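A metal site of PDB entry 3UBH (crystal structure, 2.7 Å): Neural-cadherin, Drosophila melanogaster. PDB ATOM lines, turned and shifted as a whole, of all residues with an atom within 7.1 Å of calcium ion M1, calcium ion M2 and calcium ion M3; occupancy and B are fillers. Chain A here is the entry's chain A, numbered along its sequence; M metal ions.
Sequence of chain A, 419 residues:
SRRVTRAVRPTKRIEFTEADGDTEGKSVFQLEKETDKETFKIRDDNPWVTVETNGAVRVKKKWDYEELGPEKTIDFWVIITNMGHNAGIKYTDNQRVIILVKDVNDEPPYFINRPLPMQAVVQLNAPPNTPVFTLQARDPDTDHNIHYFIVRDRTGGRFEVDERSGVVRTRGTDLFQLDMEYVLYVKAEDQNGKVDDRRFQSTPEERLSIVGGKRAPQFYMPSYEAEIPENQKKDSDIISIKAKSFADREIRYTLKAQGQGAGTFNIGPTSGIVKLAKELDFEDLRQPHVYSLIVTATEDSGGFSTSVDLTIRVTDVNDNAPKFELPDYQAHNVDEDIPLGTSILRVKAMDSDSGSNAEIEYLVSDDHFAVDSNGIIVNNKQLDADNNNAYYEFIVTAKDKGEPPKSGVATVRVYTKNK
ND2 of Asn 320 lies close to OD1 of Asp 319 (3.2 Å). The side-chain amide nitrogen (ND2) of Asn 357 lies within hydrogen-bond range of the side-chain carboxylate (OD2) of Asp 316 (3.2 Å). OD2 of Asp 316 sits at hydrogen-bond distance from N of Ser 354. ND2 of Asn 320 sits close to OE1 of Glu 283. The side-chain carboxylate (OE1) of Glu 230 lies close to the backbone NH (N) of Phe 282 (2.8 Å). The backbone NH of Glu 230 sits at hydrogen-bond distance from the backbone carbonyl oxygen of Thr 315 (3.1 Å). The backbone carbonyl oxygen (O) of Lys 406 sits at hydrogen-bond distance from the backbone NH (N) of Asp 400. The side-chain carboxylate (OD1) of Asp 400 is in hydrogen-bond range of the backbone NH (N) of Gly 402 (2.7 Å).
Of the 28 residues printed, 6 come within 4 Å of calcium ion M1.
Of the 28 residues printed, 4 come within 4 Å of calcium ion M2.
Six residues have an atom within 4 Å of calcium ion M3: Asn 318, Asn 320, Asp 351, Asp 353, Asn 357 and Asp 400.
Calcium ion M1 is bound by the side-chain carboxylate (OD1) of Asp 316 (2.2 Å), the backbone carbonyl oxygen (O) of Val 317 (2.4 Å), the side-chain carboxylate (OE2) of Glu 230 (2.4 Å), the side-chain carboxylate (OD1) of Asp 353 (2.5 Å), the side-chain carboxylate (OE1) of Glu 283 (2.5 Å), the side-chain carboxylate (OD1) of Asp 319 (2.5 Å) and the side-chain carboxylate (OE2) of Glu 283 (2.6 Å). Calcium ion M1 has seven donor atoms within binding distance.
Calcium ion M2 is bound by the side-chain carboxylate (OD2) of Asp 281 (2.1 Å), the side-chain carboxylate (OD2) of Asp 319 (2.2 Å), the side-chain carboxylate (OE1) of Glu 283 (2.5 Å) and the side-chain carboxylate (OE1) of Glu 230 (2.6 Å).
Calcium ion M3 is bound by O of Asn 357 (2.3 Å), OD1 of Asn 318 (2.3 Å), O of Asn 320 (2.3 Å), OD2 of Asp 353 (2.4 Å), OD2 of Asp 351 (2.4 Å), OD1 of Asp 351 (2.7 Å) and OD2 of Asp 400 (2.7 Å). Calcium ion M3 has seven donor atoms within binding distance.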
ATOM      1  N   GLU A 230     -18.566  -0.499  25.627  1.00  0.00           N
ATOM      2  CA  GLU A 230     -18.450  -1.824  26.252  1.00  0.00           C
ATOM      3  C   GLU A 230     -17.602  -2.837  25.480  1.00  0.00           C
ATOM      4  O   GLU A 230     -17.178  -3.853  26.048  1.00  0.00           O
ATOM      5  CB  GLU A 230     -19.850  -2.416  26.511  1.00  0.00           C
ATOM      6  CG  GLU A 230     -20.598  -2.906  25.263  1.00  0.00           C
ATOM      7  CD  GLU A 230     -21.775  -3.826  25.563  1.00  0.00           C
ATOM      8  OE1 GLU A 230     -21.710  -4.593  26.545  1.00  0.00           O
ATOM      9  OE2 GLU A 230     -22.773  -3.787  24.812  1.00  0.00           O
ATOM     10  N   ASN A 231     -17.362  -2.577  24.207  1.00  0.00           N
ATOM     11  CA  ASN A 231     -16.689  -3.550  23.366  1.00  0.00           C
ATOM     12  C   ASN A 231     -15.237  -3.196  23.094  1.00  0.00           C
ATOM     13  O   ASN A 231     -14.598  -3.799  22.220  1.00  0.00           O
ATOM     14  CB  ASN A 231     -17.434  -3.700  22.034  1.00  0.00           C
ATOM     15  CG  ASN A 231     -17.338  -2.459  21.158  1.00  0.00           C
ATOM     16  OD1 ASN A 231     -17.028  -1.348  21.628  1.00  0.00           O
ATOM     17  ND2 ASN A 231     -17.621  -2.633  19.873  1.00  0.00           N
ATOM     18  N   LEU A 280     -15.205  -5.670  29.198  1.00  0.00           N
ATOM     19  CA  LEU A 280     -16.433  -5.123  29.758  1.00  0.00           C
ATOM     20  C   LEU A 280     -17.732  -5.777  29.234  1.00  0.00           C
ATOM     21  O   LEU A 280     -17.724  -6.484  28.225  1.00  0.00           O
ATOM     22  CB  LEU A 280     -16.493  -3.619  29.536  1.00  0.00           C
ATOM     23  CG  LEU A 280     -15.321  -2.779  30.045  1.00  0.00           C
ATOM     24  CD1 LEU A 280     -15.095  -1.620  29.099  1.00  0.00           C
ATOM     25  CD2 LEU A 280     -15.587  -2.303  31.464  1.00  0.00           C
ATOM     26  N   ASP A 281     -18.844  -5.539  29.936  1.00  0.00           N
ATOM     27  CA  ASP A 281     -20.167  -6.020  29.528  1.00  0.00           C
ATOM     28  C   ASP A 281     -21.302  -5.157  30.120  1.00  0.00           C
ATOM     29  O   ASP A 281     -21.643  -5.295  31.301  1.00  0.00           O
ATOM     30  CB  ASP A 281     -20.349  -7.502  29.879  1.00  0.00           C
ATOM     31  CG  ASP A 281     -21.545  -8.131  29.176  1.00  0.00           C
ATOM     32  OD1 ASP A 281     -22.006  -9.184  29.652  1.00  0.00           O
ATOM     33  OD2 ASP A 281     -22.013  -7.592  28.158  1.00  0.00           O
ATOM     34  N   PHE A 282     -21.861  -4.288  29.292  1.00  0.00           N
ATOM     35  CA  PHE A 282     -22.998  -3.434  29.646  1.00  0.00           C
ATOM     36  C   PHE A 282     -24.177  -4.258  30.112  1.00  0.00           C
ATOM     37  O   PHE A 282     -25.012  -3.777  30.879  1.00  0.00           O
ATOM     38  CB  PHE A 282     -23.404  -2.610  28.428  1.00  0.00           C
ATOM     39  CG  PHE A 282     -24.402  -1.521  28.702  1.00  0.00           C
ATOM     40  CD1 PHE A 282     -23.979  -0.251  29.105  1.00  0.00           C
ATOM     41  CD2 PHE A 282     -25.759  -1.744  28.510  1.00  0.00           C
ATOM     42  CE1 PHE A 282     -24.895   0.768  29.331  1.00  0.00           C
ATOM     43  CE2 PHE A 282     -26.692  -0.743  28.743  1.00  0.00           C
ATOM     44  CZ  PHE A 282     -26.264   0.516  29.158  1.00  0.00           C
ATOM     45  N   GLU A 283     -24.252  -5.504  29.646  1.00  0.00           N
ATOM     46  CA  GLU A 283     -25.318  -6.431  30.005  1.00  0.00           C
ATOM     47  C   GLU A 283     -25.073  -7.168  31.326  1.00  0.00           C
ATOM     48  O   GLU A 283     -25.949  -7.865  31.837  1.00  0.00           O
ATOM     49  CB  GLU A 283     -25.561  -7.446  28.867  1.00  0.00           C
ATOM     50  CG  GLU A 283     -26.420  -6.921  27.730  1.00  0.00           C
ATOM     51  CD  GLU A 283     -25.731  -5.848  26.887  1.00  0.00           C
ATOM     52  OE1 GLU A 283     -24.675  -6.144  26.276  1.00  0.00           O
ATOM     53  OE2 GLU A 283     -26.246  -4.707  26.852  1.00  0.00           O
ATOM     54  N   ASP A 284     -23.873  -7.017  31.891  1.00  0.00           N
ATOM     55  CA  ASP A 284     -23.544  -7.682  33.149  1.00  0.00           C
ATOM     56  C   ASP A 284     -23.906  -6.797  34.338  1.00  0.00           C
ATOM     57  O   ASP A 284     -23.216  -5.812  34.633  1.00  0.00           O
ATOM     58  CB  ASP A 284     -22.065  -8.064  33.184  1.00  0.00           C
ATOM     59  CG  ASP A 284     -21.750  -9.056  34.278  1.00  0.00           C
ATOM     60  OD1 ASP A 284     -22.208  -8.862  35.421  1.00  0.00           O
ATOM     61  OD2 ASP A 284     -21.023 -10.033  33.999  1.00  0.00           O
ATOM     62  N   THR A 315     -20.838   2.504  27.600  1.00  0.00           N
ATOM     63  CA  THR A 315     -22.026   2.575  26.737  1.00  0.00           C
ATOM     64  C   THR A 315     -22.393   1.239  26.102  1.00  0.00           C
ATOM     65  O   THR A 315     -21.549   0.381  25.865  1.00  0.00           O
ATOM     66  CB  THR A 315     -21.869   3.626  25.616  1.00  0.00           C
ATOM     67  OG1 THR A 315     -20.529   3.560  25.097  1.00  0.00           O
ATOM     68  CG2 THR A 315     -22.140   5.032  26.150  1.00  0.00           C
ATOM     69  N   ASP A 316     -23.688   1.083  25.842  1.00  0.00           N
ATOM     70  CA  ASP A 316     -24.254  -0.108  25.221  1.00  0.00           C
ATOM     71  C   ASP A 316     -23.863  -0.163  23.732  1.00  0.00           C
ATOM     72  O   ASP A 316     -23.992   0.823  23.006  1.00  0.00           O
ATOM     73  CB  ASP A 316     -25.781  -0.094  25.400  1.00  0.00           C
ATOM     74  CG  ASP A 316     -26.503  -1.244  24.674  1.00  0.00           C
ATOM     75  OD1 ASP A 316     -25.986  -2.380  24.630  1.00  0.00           O
ATOM     76  OD2 ASP A 316     -27.614  -0.999  24.161  1.00  0.00           O
ATOM     77  N   VAL A 317     -23.368  -1.317  23.293  1.00  0.00           N
ATOM     78  CA  VAL A 317     -23.274  -1.603  21.864  1.00  0.00           C
ATOM     79  C   VAL A 317     -24.217  -2.745  21.551  1.00  0.00           C
ATOM     80  O   VAL A 317     -24.555  -3.555  22.433  1.00  0.00           O
ATOM     81  CB  VAL A 317     -21.824  -1.916  21.374  1.00  0.00           C
ATOM     82  CG1 VAL A 317     -20.832  -0.878  21.925  1.00  0.00           C
ATOM     83  CG2 VAL A 317     -21.400  -3.351  21.719  1.00  0.00           C
ATOM     84  N   ASN A 318     -24.664  -2.811  20.308  1.00  0.00           N
ATOM     85  CA  ASN A 318     -25.593  -3.841  19.881  1.00  0.00           C
ATOM     86  C   ASN A 318     -24.866  -5.169  19.699  1.00  0.00           C
ATOM     87  O   ASN A 318     -24.700  -5.638  18.573  1.00  0.00           O
ATOM     88  CB  ASN A 318     -26.320  -3.415  18.599  1.00  0.00           C
ATOM     89  CG  ASN A 318     -27.441  -4.359  18.220  1.00  0.00           C
ATOM     90  OD1 ASN A 318     -28.256  -4.754  19.059  1.00  0.00           O
ATOM     91  ND2 ASN A 318     -27.489  -4.732  16.937  1.00  0.00           N
ATOM     92  N   ASP A 319     -24.423  -5.754  20.799  1.00  0.00           N
ATOM     93  CA  ASP A 319     -23.722  -7.051  20.747  1.00  0.00           C
ATOM     94  C   ASP A 319     -24.657  -8.251  20.920  1.00  0.00           C
ATOM     95  O   ASP A 319     -24.211  -9.396  20.911  1.00  0.00           O
ATOM     96  CB  ASP A 319     -22.510  -7.112  21.716  1.00  0.00           C
ATOM     97  CG  ASP A 319     -22.855  -6.686  23.143  1.00  0.00           C
ATOM     98  OD1 ASP A 319     -24.011  -6.342  23.434  1.00  0.00           O
ATOM     99  OD2 ASP A 319     -21.930  -6.672  23.996  1.00  0.00           O
ATOM    100  N   ASN A 320     -25.953  -8.002  21.067  1.00  0.00           N
ATOM    101  CA  ASN A 320     -26.900  -9.101  21.250  1.00  0.00           C
ATOM    102  C   ASN A 320     -27.963  -9.205  20.175  1.00  0.00           C
ATOM    103  O   ASN A 320     -28.554  -8.202  19.767  1.00  0.00           O
ATOM    104  CB  ASN A 320     -27.514  -9.050  22.640  1.00  0.00           C
ATOM    105  CG  ASN A 320     -26.582  -9.558  23.707  1.00  0.00           C
ATOM    106  OD1 ASN A 320     -26.374 -10.769  23.843  1.00  0.00           O
ATOM    107  ND2 ASN A 320     -25.986  -8.641  24.469  1.00  0.00           N
ATOM    108  N   ALA A 321     -28.205 -10.423  19.710  1.00  0.00           N
ATOM    109  CA  ALA A 321     -29.296 -10.681  18.772  1.00  0.00           C
ATOM    110  C   ALA A 321     -30.576 -11.095  19.499  1.00  0.00           C
ATOM    111  O   ALA A 321     -30.519 -11.740  20.559  1.00  0.00           O
ATOM    112  CB  ALA A 321     -28.872 -11.739  17.758  1.00  0.00           C
ATOM    113  N   PRO A 322     -31.754 -10.707  18.957  1.00  0.00           N
ATOM    114  CA  PRO A 322     -33.019 -11.159  19.569  1.00  0.00           C
ATOM    115  C   PRO A 322     -33.070 -12.691  19.633  1.00  0.00           C
ATOM    116  O   PRO A 322     -32.714 -13.337  18.646  1.00  0.00           O
ATOM    117  CB  PRO A 322     -34.086 -10.638  18.590  1.00  0.00           C
ATOM    118  CG  PRO A 322     -33.443  -9.472  17.904  1.00  0.00           C
ATOM    119  CD  PRO A 322     -31.993  -9.835  17.787  1.00  0.00           C
ATOM    120  N   ASP A 351     -34.261  -9.532  23.679  1.00  0.00           N
ATOM    121  CA  ASP A 351     -32.963  -8.966  23.312  1.00  0.00           C
ATOM    122  C   ASP A 351     -32.321  -8.326  24.544  1.00  0.00           C
ATOM    123  O   ASP A 351     -32.928  -7.463  25.181  1.00  0.00           O
ATOM    124  CB  ASP A 351     -33.147  -7.924  22.198  1.00  0.00           C
ATOM    125  CG  ASP A 351     -31.835  -7.509  21.525  1.00  0.00           C
ATOM    126  OD1 ASP A 351     -30.793  -7.339  22.217  1.00  0.00           O
ATOM    127  OD2 ASP A 351     -31.829  -7.325  20.287  1.00  0.00           O
ATOM    128  N   SER A 352     -31.104  -8.754  24.852  1.00  0.00           N
ATOM    129  CA  SER A 352     -30.346  -8.302  26.035  1.00  0.00           C
ATOM    130  C   SER A 352     -29.966  -6.815  26.067  1.00  0.00           C
ATOM    131  O   SER A 352     -29.785  -6.251  27.149  1.00  0.00           O
ATOM    132  CB  SER A 352     -29.048  -9.095  26.156  1.00  0.00           C
ATOM    133  OG  SER A 352     -29.315 -10.462  26.369  1.00  0.00           O
ATOM    134  N   ASP A 353     -29.799  -6.202  24.899  1.00  0.00           N
ATOM    135  CA  ASP A 353     -29.311  -4.833  24.785  1.00  0.00           C
ATOM    136  C   ASP A 353     -30.330  -3.820  25.309  1.00  0.00           C
ATOM    137  O   ASP A 353     -31.357  -4.205  25.884  1.00  0.00           O
ATOM    138  CB  ASP A 353     -28.930  -4.510  23.327  1.00  0.00           C
ATOM    139  CG  ASP A 353     -27.884  -5.477  22.778  1.00  0.00           C
ATOM    140  OD1 ASP A 353     -26.869  -5.722  23.460  1.00  0.00           O
ATOM    141  OD2 ASP A 353     -28.060  -5.976  21.648  1.00  0.00           O
ATOM    142  N   SER A 354     -30.048  -2.532  25.140  1.00  0.00           N
ATOM    143  CA  SER A 354     -30.938  -1.483  25.648  1.00  0.00           C
ATOM    144  C   SER A 354     -31.441  -0.554  24.550  1.00  0.00           C
ATOM    145  O   SER A 354     -31.010  -0.650  23.403  1.00  0.00           O
ATOM    146  CB  SER A 354     -30.245  -0.728  26.756  1.00  0.00           C
ATOM    147  OG  SER A 354     -29.764  -1.656  27.698  1.00  0.00           O
ATOM    148  N   SER A 356     -33.004   1.135  21.510  1.00  0.00           N
ATOM    149  CA  SER A 356     -33.372   0.603  20.208  1.00  0.00           C
ATOM    150  C   SER A 356     -32.528  -0.588  19.747  1.00  0.00           C
ATOM    151  O   SER A 356     -32.912  -1.301  18.800  1.00  0.00           O
ATOM    152  CB  SER A 356     -33.380   1.706  19.142  1.00  0.00           C
ATOM    153  OG  SER A 356     -32.092   2.242  18.972  1.00  0.00           O
ATOM    154  N   ASN A 357     -31.398  -0.822  20.404  1.00  0.00           N
ATOM    155  CA  ASN A 357     -30.643  -2.067  20.174  1.00  0.00           C
ATOM    156  C   ASN A 357     -31.433  -3.263  20.699  1.00  0.00           C
ATOM    157  O   ASN A 357     -31.075  -4.410  20.426  1.00  0.00           O
ATOM    158  CB  ASN A 357     -29.266  -2.023  20.833  1.00  0.00           C
ATOM    159  CG  ASN A 357     -28.319  -1.005  20.228  1.00  0.00           C
ATOM    160  OD1 ASN A 357     -28.340  -0.719  19.029  1.00  0.00           O
ATOM    161  ND2 ASN A 357     -27.451  -0.470  21.060  1.00  0.00           N
ATOM    162  N   ALA A 358     -32.495  -2.995  21.444  1.00  0.00           N
ATOM    163  CA  ALA A 358     -33.421  -4.020  21.952  1.00  0.00           C
ATOM    164  C   ALA A 358     -34.848  -3.907  21.395  1.00  0.00           C
ATOM    165  O   ALA A 358     -35.736  -4.678  21.766  1.00  0.00           O
ATOM    166  CB  ALA A 358     -33.444  -3.985  23.471  1.00  0.00           C
ATOM    167  N   GLU A 359     -35.077  -2.936  20.512  1.00  0.00           N
ATOM    168  CA  GLU A 359     -36.372  -2.742  19.881  1.00  0.00           C
ATOM    169  C   GLU A 359     -36.554  -3.813  18.807  1.00  0.00           C
ATOM    170  O   GLU A 359     -35.681  -4.010  17.971  1.00  0.00           O
ATOM    171  CB  GLU A 359     -36.429  -1.350  19.239  1.00  0.00           C
ATOM    172  CG  GLU A 359     -37.829  -0.791  19.035  1.00  0.00           C
ATOM    173  CD  GLU A 359     -38.321   0.018  20.220  1.00  0.00           C
ATOM    174  OE1 GLU A 359     -39.552  -0.010  20.469  1.00  0.00           O
ATOM    175  OE2 GLU A 359     -37.502   0.672  20.903  1.00  0.00           O
ATOM    176  N   ASP A 400     -33.739  -6.520  15.413  1.00  0.00           N
ATOM    177  CA  ASP A 400     -33.638  -5.337  16.254  1.00  0.00           C
ATOM    178  C   ASP A 400     -33.436  -4.070  15.435  1.00  0.00           C
ATOM    179  O   ASP A 400     -33.270  -4.124  14.215  1.00  0.00           O
ATOM    180  CB  ASP A 400     -32.574  -5.488  17.376  1.00  0.00           C
ATOM    181  CG  ASP A 400     -31.138  -5.467  16.852  1.00  0.00           C
ATOM    182  OD1 ASP A 400     -30.822  -4.688  15.925  1.00  0.00           O
ATOM    183  OD2 ASP A 400     -30.312  -6.222  17.389  1.00  0.00           O
ATOM    184  N   LYS A 401     -33.442  -2.924  16.116  1.00  0.00           N
ATOM    185  CA  LYS A 401     -33.241  -1.632  15.446  1.00  0.00           C
ATOM    186  C   LYS A 401     -31.838  -1.060  15.687  1.00  0.00           C
ATOM    187  O   LYS A 401     -31.641   0.153  15.702  1.00  0.00           O
ATOM    188  CB  LYS A 401     -34.329  -0.632  15.853  1.00  0.00           C
ATOM    189  CG  LYS A 401     -35.756  -1.046  15.473  1.00  0.00           C
ATOM    190  CD  LYS A 401     -36.713   0.156  15.451  1.00  0.00           C
ATOM    191  CE  LYS A 401     -38.179  -0.266  15.434  1.00  0.00           C
ATOM    192  NZ  LYS A 401     -38.511  -1.158  14.281  1.00  0.00           N
ATOM    193  N   GLY A 402     -30.867  -1.964  15.861  1.00  0.00           N
ATOM    194  CA  GLY A 402     -29.466  -1.565  16.047  1.00  0.00           C
ATOM    195  C   GLY A 402     -28.794  -1.173  14.748  1.00  0.00           C
ATOM    196  O   GLY A 402     -29.364  -1.313  13.672  1.00  0.00           O
ATOM    197  N   PRO A 405     -28.357  -3.824  12.314  1.00  0.00           N
ATOM    198  CA  PRO A 405     -29.311  -4.653  13.043  1.00  0.00           C
ATOM    199  C   PRO A 405     -28.947  -6.134  13.070  1.00  0.00           C
ATOM    200  O   PRO A 405     -28.541  -6.693  12.056  1.00  0.00           O
ATOM    201  CB  PRO A 405     -30.627  -4.439  12.266  1.00  0.00           C
ATOM    202  CG  PRO A 405     -30.208  -4.130  10.888  1.00  0.00           C
ATOM    203  CD  PRO A 405     -28.890  -3.400  10.997  1.00  0.00           C
ATOM    204  N   LYS A 406     -29.103  -6.755  14.243  1.00  0.00           N
ATOM    205  CA  LYS A 406     -28.888  -8.196  14.414  1.00  0.00           C
ATOM    206  C   LYS A 406     -30.230  -8.934  14.364  1.00  0.00           C
ATOM    207  O   LYS A 406     -31.260  -8.364  14.713  1.00  0.00           O
ATOM    208  CB  LYS A 406     -28.179  -8.477  15.749  1.00  0.00           C
ATOM    209  CG  LYS A 406     -26.757  -7.922  15.834  1.00  0.00           C
ATOM    210  CD  LYS A 406     -25.813  -8.929  16.499  1.00  0.00           C
ATOM    211  CE  LYS A 406     -24.468  -8.325  16.859  1.00  0.00           C
ATOM    212  NZ  LYS A 406     -23.732  -7.774  15.686  1.00  0.00           N
HETATM  213 CA    CA M   1     -25.116  -4.399  24.557  1.00  0.00          CA
HETATM  214 CA    CA M   2     -22.312  -7.066  26.105  1.00  0.00          CA
HETATM  215 CA    CA M   3     -29.753  -6.224  20.034  1.00  0.00          CA
